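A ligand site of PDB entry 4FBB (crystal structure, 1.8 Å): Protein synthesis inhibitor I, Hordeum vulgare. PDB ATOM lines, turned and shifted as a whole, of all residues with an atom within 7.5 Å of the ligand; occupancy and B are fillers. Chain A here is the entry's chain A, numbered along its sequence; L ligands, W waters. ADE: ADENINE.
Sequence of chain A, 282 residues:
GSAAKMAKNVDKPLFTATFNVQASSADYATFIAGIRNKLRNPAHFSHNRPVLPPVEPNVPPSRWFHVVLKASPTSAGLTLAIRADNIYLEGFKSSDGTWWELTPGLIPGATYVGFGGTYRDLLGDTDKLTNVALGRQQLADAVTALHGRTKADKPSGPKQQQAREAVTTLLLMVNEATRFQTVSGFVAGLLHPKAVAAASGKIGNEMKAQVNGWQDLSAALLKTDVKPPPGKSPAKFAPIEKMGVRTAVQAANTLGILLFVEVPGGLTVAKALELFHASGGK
The side-chain carboxylate (OE2) of Glu 176 lies within hydrogen-bond range of a nitrogen (N9) of the ligand (3.2 Å).
A nitrogen (N1) of the ligand is in hydrogen-bond range of the backbone NH of Leu 89 (3.0 Å).
A nitrogen (N6) of the ligand sits at hydrogen-bond distance from the backbone carbonyl oxygen of Gly 117 (2.4 Å).
NH1 of Arg 179 lies within hydrogen-bond range of N3 of the ligand, 3.1 Å away.
Ile 87 touches the ligand (O to C2, 3.7 Å).
CD2 of Tyr 88 touches N1 of the ligand, 3.3 Å away.
CA of Thr 118 touches N7 of the ligand (3.8 Å).
Tyr 119 touches the ligand.
Leu 171 touches the ligand (CD2 to N1, 3.6 Å).
Nine residues have an atom within 4 Å of the ligand: Ile 87, Tyr 88, Leu 89, Gly 117, Thr 118, Tyr 119, Leu 171, Glu 176 and Arg 179.
The nearest printed residue that does not touch the ligand is Asn 175 (4.4 Å).
O of Leu 171 sits at hydrogen-bond distance from N of Glu 176 (2.7 Å).
O of Ile 87 is in hydrogen-bond range of NH2 of Arg 179, 3.1 Å away.
N of Tyr 88 sits close to OD1 of Asn 86 (3.3 Å).
NH1 of Arg 179 lies within salt-bridge range of OE2 of Glu 176 (3.1 Å).
The backbone carbonyl oxygen of Ile 87 lies within hydrogen-bond range of the side-chain amide nitrogen of Asn 175.
OE2 of Glu 176 is in hydrogen-bond range of OH of Tyr 119, at 2.7 Å.
The backbone carbonyl oxygen of Asn 86 sits at hydrogen-bond distance from the guanidinium group of Arg 179, at 2.8 Å.
The side-chain hydroxyl of Thr 118 sits at hydrogen-bond distance from the side-chain carboxylate of Asp 121.
Water W1 lies within hydrogen-bond range of a nitrogen (N9) of the ligand (2.8 Å), the side-chain carboxylate (OE2) of Glu 176 (3.0 Å) and the backbone carbonyl oxygen (O) of Val 211 (3.3 Å).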
ATOM      1  N   ALA A  81      32.679  12.649 -15.809  1.00  0.00           N
ATOM      2  CA  ALA A  81      32.755  13.723 -16.793  1.00  0.00           C
ATOM      3  C   ALA A  81      32.184  15.002 -16.191  1.00  0.00           C
ATOM      4  O   ALA A  81      30.988  15.084 -15.898  1.00  0.00           O
ATOM      5  CB  ALA A  81      31.983  13.359 -18.045  1.00  0.00           C
ATOM      6  N   ILE A  82      33.051  15.990 -16.000  1.00  0.00           N
ATOM      7  CA  ILE A  82      32.700  17.177 -15.234  1.00  0.00           C
ATOM      8  C   ILE A  82      33.065  18.429 -16.018  1.00  0.00           C
ATOM      9  O   ILE A  82      34.122  18.472 -16.658  1.00  0.00           O
ATOM     10  CB  ILE A  82      33.471  17.187 -13.897  1.00  0.00           C
ATOM     11  CG1 ILE A  82      33.241  15.873 -13.136  1.00  0.00           C
ATOM     12  CG2 ILE A  82      33.051  18.355 -13.049  1.00  0.00           C
ATOM     13  CD1 ILE A  82      34.192  15.661 -11.968  1.00  0.00           C
ATOM     14  N   ASN A  86      31.851  25.185 -14.416  1.00  0.00           N
ATOM     15  CA  ASN A  86      31.042  25.226 -13.202  1.00  0.00           C
ATOM     16  C   ASN A  86      31.071  23.932 -12.390  1.00  0.00           C
ATOM     17  O   ASN A  86      30.275  23.769 -11.455  1.00  0.00           O
ATOM     18  CB  ASN A  86      29.582  25.610 -13.512  1.00  0.00           C
ATOM     19  CG  ASN A  86      28.870  24.561 -14.344  1.00  0.00           C
ATOM     20  OD1 ASN A  86      29.464  23.591 -14.820  1.00  0.00           O
ATOM     21  ND2 ASN A  86      27.568  24.777 -14.565  1.00  0.00           N
ATOM     22  N   ILE A  87      31.968  23.028 -12.769  1.00  0.00           N
ATOM     23  CA  ILE A  87      32.206  21.779 -12.036  1.00  0.00           C
ATOM     24  C   ILE A  87      30.937  20.927 -11.948  1.00  0.00           C
ATOM     25  O   ILE A  87      30.692  20.237 -10.947  1.00  0.00           O
ATOM     26  CB  ILE A  87      32.839  22.048 -10.658  1.00  0.00           C
ATOM     27  CG1 ILE A  87      33.894  23.164 -10.770  1.00  0.00           C
ATOM     28  CG2 ILE A  87      33.521  20.784 -10.135  1.00  0.00           C
ATOM     29  CD1 ILE A  87      34.395  23.698  -9.411  1.00  0.00           C
ATOM     30  N   TYR A  88      30.132  20.961 -12.999  1.00  0.00           N
ATOM     31  CA  TYR A  88      28.930  20.156 -13.024  1.00  0.00           C
ATOM     32  C   TYR A  88      29.187  18.745 -13.527  1.00  0.00           C
ATOM     33  O   TYR A  88      29.877  18.529 -14.535  1.00  0.00           O
ATOM     34  CB  TYR A  88      27.792  20.850 -13.809  1.00  0.00           C
ATOM     35  CG  TYR A  88      26.803  21.471 -12.857  1.00  0.00           C
ATOM     36  CD1 TYR A  88      27.106  22.657 -12.195  1.00  0.00           C
ATOM     37  CD2 TYR A  88      25.599  20.853 -12.580  1.00  0.00           C
ATOM     38  CE1 TYR A  88      26.216  23.213 -11.303  1.00  0.00           C
ATOM     39  CE2 TYR A  88      24.701  21.398 -11.679  1.00  0.00           C
ATOM     40  CZ  TYR A  88      25.011  22.582 -11.056  1.00  0.00           C
ATOM     41  OH  TYR A  88      24.121  23.138 -10.165  1.00  0.00           O
ATOM     42  N   LEU A  89      28.660  17.768 -12.788  1.00  0.00           N
ATOM     43  CA  LEU A  89      28.782  16.375 -13.193  1.00  0.00           C
ATOM     44  C   LEU A  89      27.629  16.085 -14.128  1.00  0.00           C
ATOM     45  O   LEU A  89      26.464  16.285 -13.767  1.00  0.00           O
ATOM     46  CB  LEU A  89      28.715  15.421 -11.992  1.00  0.00           C
ATOM     47  CG  LEU A  89      28.701  13.934 -12.373  1.00  0.00           C
ATOM     48  CD1 LEU A  89      29.963  13.550 -13.122  1.00  0.00           C
ATOM     49  CD2 LEU A  89      28.503  13.030 -11.157  1.00  0.00           C
ATOM     50  N   GLU A  90      27.953  15.622 -15.323  1.00  0.00           N
ATOM     51  CA  GLU A  90      26.941  15.349 -16.327  1.00  0.00           C
ATOM     52  C   GLU A  90      27.019  13.921 -16.859  1.00  0.00           C
ATOM     53  O   GLU A  90      26.024  13.394 -17.376  1.00  0.00           O
ATOM     54  CB  GLU A  90      27.020  16.354 -17.479  1.00  0.00           C
ATOM     55  CG  GLU A  90      26.480  17.738 -17.133  1.00  0.00           C
ATOM     56  CD  GLU A  90      25.003  17.703 -16.777  1.00  0.00           C
ATOM     57  OE1 GLU A  90      24.318  16.730 -17.162  1.00  0.00           O
ATOM     58  OE2 GLU A  90      24.512  18.656 -16.120  1.00  0.00           O
ATOM     59  N   LEU A 102      23.430  12.388 -17.245  1.00  0.00           N
ATOM     60  CA  LEU A 102      22.449  12.847 -16.270  1.00  0.00           C
ATOM     61  C   LEU A 102      21.512  13.893 -16.862  1.00  0.00           C
ATOM     62  O   LEU A 102      20.557  14.347 -16.189  1.00  0.00           O
ATOM     63  CB  LEU A 102      23.158  13.370 -15.019  1.00  0.00           C
ATOM     64  CG  LEU A 102      23.848  12.264 -14.210  1.00  0.00           C
ATOM     65  CD1 LEU A 102      24.925  12.787 -13.252  1.00  0.00           C
ATOM     66  CD2 LEU A 102      22.802  11.483 -13.428  1.00  0.00           C
ATOM     67  N   THR A 103      21.787  14.263 -18.111  1.00  0.00           N
ATOM     68  CA  THR A 103      20.910  15.125 -18.915  1.00  0.00           C
ATOM     69  C   THR A 103      20.620  14.459 -20.260  1.00  0.00           C
ATOM     70  O   THR A 103      21.546  14.106 -20.986  1.00  0.00           O
ATOM     71  CB  THR A 103      21.569  16.485 -19.200  1.00  0.00           C
ATOM     72  OG1 THR A 103      22.011  17.074 -17.967  1.00  0.00           O
ATOM     73  CG2 THR A 103      20.606  17.428 -19.922  1.00  0.00           C
ATOM     74  N   GLY A 116      17.806  12.834 -13.103  1.00  0.00           N
ATOM     75  CA  GLY A 116      18.538  14.082 -13.257  1.00  0.00           C
ATOM     76  C   GLY A 116      19.674  14.250 -12.265  1.00  0.00           C
ATOM     77  O   GLY A 116      19.774  13.499 -11.294  1.00  0.00           O
ATOM     78  N   GLY A 117      20.520  15.246 -12.516  1.00  0.00           N
ATOM     79  CA  GLY A 117      21.712  15.461 -11.701  1.00  0.00           C
ATOM     80  C   GLY A 117      21.516  16.390 -10.526  1.00  0.00           C
ATOM     81  O   GLY A 117      22.448  16.618  -9.745  1.00  0.00           O
ATOM     82  N   THR A 118      20.319  16.943 -10.376  1.00  0.00           N
ATOM     83  CA  THR A 118      20.048  17.904  -9.307  1.00  0.00           C
ATOM     84  C   THR A 118      19.747  17.171  -7.998  1.00  0.00           C
ATOM     85  O   THR A 118      19.234  16.046  -7.998  1.00  0.00           O
ATOM     86  CB  THR A 118      18.851  18.816  -9.669  1.00  0.00           C
ATOM     87  OG1 THR A 118      19.001  19.310 -11.008  1.00  0.00           O
ATOM     88  CG2 THR A 118      18.762  20.009  -8.707  1.00  0.00           C
ATOM     89  N   TYR A 119      20.056  17.808  -6.871  1.00  0.00           N
ATOM     90  CA  TYR A 119      19.714  17.231  -5.569  1.00  0.00           C
ATOM     91  C   TYR A 119      18.207  16.949  -5.405  1.00  0.00           C
ATOM     92  O   TYR A 119      17.821  15.991  -4.735  1.00  0.00           O
ATOM     93  CB  TYR A 119      20.264  18.095  -4.437  1.00  0.00           C
ATOM     94  CG  TYR A 119      21.773  18.009  -4.362  1.00  0.00           C
ATOM     95  CD1 TYR A 119      22.423  16.793  -4.559  1.00  0.00           C
ATOM     96  CD2 TYR A 119      22.552  19.136  -4.114  1.00  0.00           C
ATOM     97  CE1 TYR A 119      23.810  16.705  -4.504  1.00  0.00           C
ATOM     98  CE2 TYR A 119      23.936  19.057  -4.061  1.00  0.00           C
ATOM     99  CZ  TYR A 119      24.556  17.834  -4.252  1.00  0.00           C
ATOM    100  OH  TYR A 119      25.926  17.763  -4.191  1.00  0.00           O
ATOM    101  N   ARG A 120      17.359  17.765  -6.038  1.00  0.00           N
ATOM    102  CA  ARG A 120      15.931  17.475  -6.044  1.00  0.00           C
ATOM    103  C   ARG A 120      15.645  16.193  -6.860  1.00  0.00           C
ATOM    104  O   ARG A 120      14.859  15.336  -6.426  1.00  0.00           O
ATOM    105  CB  ARG A 120      15.107  18.674  -6.546  1.00  0.00           C
ATOM    106  CG  ARG A 120      15.438  19.154  -7.955  1.00  0.00           C
ATOM    107  CD  ARG A 120      14.756  20.470  -8.289  1.00  0.00           C
ATOM    108  NE  ARG A 120      14.986  20.886  -9.670  1.00  0.00           N
ATOM    109  CZ  ARG A 120      15.894  21.801 -10.047  1.00  0.00           C
ATOM    110  NH1 ARG A 120      16.654  22.403  -9.147  1.00  0.00           N
ATOM    111  NH2 ARG A 120      16.025  22.100 -11.325  1.00  0.00           N
ATOM    112  N   ASP A 121      16.325  16.045  -7.996  1.00  0.00           N
ATOM    113  CA  ASP A 121      16.219  14.830  -8.807  1.00  0.00           C
ATOM    114  C   ASP A 121      16.691  13.590  -8.046  1.00  0.00           C
ATOM    115  O   ASP A 121      15.982  12.577  -7.985  1.00  0.00           O
ATOM    116  CB  ASP A 121      17.059  14.945 -10.086  1.00  0.00           C
ATOM    117  CG  ASP A 121      16.569  16.036 -11.023  1.00  0.00           C
ATOM    118  OD1 ASP A 121      15.336  16.209 -11.139  1.00  0.00           O
ATOM    119  OD2 ASP A 121      17.420  16.714 -11.638  1.00  0.00           O
ATOM    120  N   LEU A 122      17.888  13.678  -7.456  1.00  0.00           N
ATOM    121  CA  LEU A 122      18.555  12.534  -6.841  1.00  0.00           C
ATOM    122  C   LEU A 122      17.935  12.150  -5.497  1.00  0.00           C
ATOM    123  O   LEU A 122      17.637  10.982  -5.245  1.00  0.00           O
ATOM    124  CB  LEU A 122      20.032  12.847  -6.646  1.00  0.00           C
ATOM    125  CG  LEU A 122      20.826  13.160  -7.906  1.00  0.00           C
ATOM    126  CD1 LEU A 122      22.154  13.775  -7.542  1.00  0.00           C
ATOM    127  CD2 LEU A 122      21.034  11.918  -8.743  1.00  0.00           C
ATOM    128  N   LEU A 129      20.184  16.686   1.953  1.00  0.00           N
ATOM    129  CA  LEU A 129      21.648  16.532   1.893  1.00  0.00           C
ATOM    130  C   LEU A 129      22.265  16.108   3.223  1.00  0.00           C
ATOM    131  O   LEU A 129      23.253  15.376   3.254  1.00  0.00           O
ATOM    132  CB  LEU A 129      22.321  17.833   1.410  1.00  0.00           C
ATOM    133  CG  LEU A 129      22.280  18.115  -0.089  1.00  0.00           C
ATOM    134  CD1 LEU A 129      22.805  19.513  -0.389  1.00  0.00           C
ATOM    135  CD2 LEU A 129      23.055  17.066  -0.865  1.00  0.00           C
ATOM    136  N   VAL A 167      25.399   8.649  -7.116  1.00  0.00           N
ATOM    137  CA  VAL A 167      25.713   9.964  -7.669  1.00  0.00           C
ATOM    138  C   VAL A 167      25.692  11.032  -6.586  1.00  0.00           C
ATOM    139  O   VAL A 167      26.587  11.876  -6.533  1.00  0.00           O
ATOM    140  CB  VAL A 167      24.773  10.334  -8.847  1.00  0.00           C
ATOM    141  CG1 VAL A 167      24.909  11.813  -9.207  1.00  0.00           C
ATOM    142  CG2 VAL A 167      25.104   9.467 -10.054  1.00  0.00           C
ATOM    143  N   LEU A 171      28.977  13.330  -5.896  1.00  0.00           N
ATOM    144  CA  LEU A 171      28.829  14.771  -6.037  1.00  0.00           C
ATOM    145  C   LEU A 171      29.349  15.445  -4.776  1.00  0.00           C
ATOM    146  O   LEU A 171      30.044  16.466  -4.829  1.00  0.00           O
ATOM    147  CB  LEU A 171      27.360  15.157  -6.216  1.00  0.00           C
ATOM    148  CG  LEU A 171      26.713  14.887  -7.566  1.00  0.00           C
ATOM    149  CD1 LEU A 171      25.284  15.408  -7.555  1.00  0.00           C
ATOM    150  CD2 LEU A 171      27.506  15.548  -8.677  1.00  0.00           C
ATOM    151  N   ASN A 175      32.701  16.688  -6.209  1.00  0.00           N
ATOM    152  CA  ASN A 175      32.337  18.013  -6.724  1.00  0.00           C
ATOM    153  C   ASN A 175      32.200  19.091  -5.650  1.00  0.00           C
ATOM    154  O   ASN A 175      32.820  20.149  -5.760  1.00  0.00           O
ATOM    155  CB  ASN A 175      31.062  17.929  -7.571  1.00  0.00           C
ATOM    156  CG  ASN A 175      31.203  16.958  -8.723  1.00  0.00           C
ATOM    157  OD1 ASN A 175      31.189  15.741  -8.532  1.00  0.00           O
ATOM    158  ND2 ASN A 175      31.353  17.497  -9.932  1.00  0.00           N
ATOM    159  N   GLU A 176      31.388  18.820  -4.630  1.00  0.00           N
ATOM    160  CA  GLU A 176      31.169  19.792  -3.583  1.00  0.00           C
ATOM    161  C   GLU A 176      32.470  19.959  -2.788  1.00  0.00           C
ATOM    162  O   GLU A 176      32.770  21.046  -2.272  1.00  0.00           O
ATOM    163  CB  GLU A 176      30.009  19.367  -2.682  1.00  0.00           C
ATOM    164  CG  GLU A 176      28.712  19.049  -3.446  1.00  0.00           C
ATOM    165  CD  GLU A 176      28.153  20.242  -4.239  1.00  0.00           C
ATOM    166  OE1 GLU A 176      28.648  21.390  -4.090  1.00  0.00           O
ATOM    167  OE2 GLU A 176      27.213  20.020  -5.041  1.00  0.00           O
ATOM    168  N   ARG A 179      34.563  22.447  -4.626  1.00  0.00           N
ATOM    169  CA  ARG A 179      34.020  23.788  -4.389  1.00  0.00           C
ATOM    170  C   ARG A 179      34.239  24.329  -2.977  1.00  0.00           C
ATOM    171  O   ARG A 179      34.446  25.530  -2.819  1.00  0.00           O
ATOM    172  CB  ARG A 179      32.529  23.814  -4.681  1.00  0.00           C
ATOM    173  CG  ARG A 179      32.199  23.674  -6.149  1.00  0.00           C
ATOM    174  CD  ARG A 179      30.788  23.166  -6.290  1.00  0.00           C
ATOM    175  NE  ARG A 179      30.350  23.111  -7.680  1.00  0.00           N
ATOM    176  CZ  ARG A 179      29.339  22.362  -8.104  1.00  0.00           C
ATOM    177  NH1 ARG A 179      28.684  21.595  -7.237  1.00  0.00           N
ATOM    178  NH2 ARG A 179      28.994  22.373  -9.391  1.00  0.00           N
ATOM    179  N   VAL A 211      26.557  24.450   0.112  1.00  0.00           N
ATOM    180  CA  VAL A 211      26.400  23.704  -1.135  1.00  0.00           C
ATOM    181  C   VAL A 211      25.241  24.250  -1.995  1.00  0.00           C
ATOM    182  O   VAL A 211      25.325  24.313  -3.235  1.00  0.00           O
ATOM    183  CB  VAL A 211      26.205  22.189  -0.873  1.00  0.00           C
ATOM    184  CG1 VAL A 211      25.759  21.473  -2.129  1.00  0.00           C
ATOM    185  CG2 VAL A 211      27.502  21.567  -0.371  1.00  0.00           C
ATOM    186  N   ASN A 212      24.169  24.673  -1.328  1.00  0.00           N
ATOM    187  CA  ASN A 212      22.994  25.191  -2.036  1.00  0.00           C
ATOM    188  C   ASN A 212      23.118  26.676  -2.399  1.00  0.00           C
ATOM    189  O   ASN A 212      22.245  27.230  -3.090  1.00  0.00           O
ATOM    190  CB  ASN A 212      21.718  24.935  -1.226  1.00  0.00           C
ATOM    191  CG  ASN A 212      21.362  23.453  -1.136  1.00  0.00           C
ATOM    192  OD1 ASN A 212      21.583  22.690  -2.085  1.00  0.00           O
ATOM    193  ND2 ASN A 212      20.788  23.058  -0.007  1.00  0.00           N
ATOM    194  N   TRP A 214      26.397  28.230  -3.479  1.00  0.00           N
ATOM    195  CA  TRP A 214      27.746  28.411  -4.008  1.00  0.00           C
ATOM    196  C   TRP A 214      27.856  29.713  -4.787  1.00  0.00           C
ATOM    197  O   TRP A 214      28.794  30.470  -4.590  1.00  0.00           O
ATOM    198  CB  TRP A 214      28.122  27.246  -4.914  1.00  0.00           C
ATOM    199  CG  TRP A 214      29.557  27.278  -5.479  1.00  0.00           C
ATOM    200  CD1 TRP A 214      30.697  27.659  -4.826  1.00  0.00           C
ATOM    201  CD2 TRP A 214      29.967  26.875  -6.796  1.00  0.00           C
ATOM    202  NE1 TRP A 214      31.789  27.523  -5.661  1.00  0.00           N
ATOM    203  CE2 TRP A 214      31.368  27.036  -6.868  1.00  0.00           C
ATOM    204  CE3 TRP A 214      29.279  26.393  -7.905  1.00  0.00           C
ATOM    205  CZ2 TRP A 214      32.084  26.728  -8.028  1.00  0.00           C
ATOM    206  CZ3 TRP A 214      29.992  26.087  -9.046  1.00  0.00           C
ATOM    207  CH2 TRP A 214      31.386  26.267  -9.109  1.00  0.00           C
HETATM  208  N9  ADE L   1      25.255  20.140  -7.571  1.00  0.00           N
HETATM  209  C8  ADE L   1      23.982  19.659  -7.497  1.00  0.00           C
HETATM  210  N7  ADE L   1      23.684  18.814  -8.466  1.00  0.00           N
HETATM  211  C5  ADE L   1      24.840  18.745  -9.213  1.00  0.00           C
HETATM  212  C6  ADE L   1      25.195  18.034 -10.377  1.00  0.00           C
HETATM  213  N6  ADE L   1      24.385  17.216 -11.047  1.00  0.00           N
HETATM  214  N1  ADE L   1      26.442  18.215 -10.861  1.00  0.00           N
HETATM  215  C2  ADE L   1      27.287  19.038 -10.226  1.00  0.00           C
HETATM  216  N3  ADE L   1      27.076  19.757  -9.131  1.00  0.00           N
HETATM  217  C4  ADE L   1      25.816  19.569  -8.689  1.00  0.00           C
HETATM  218  O   HOH W   1      25.120  22.091  -5.630  1.00  0.00           O
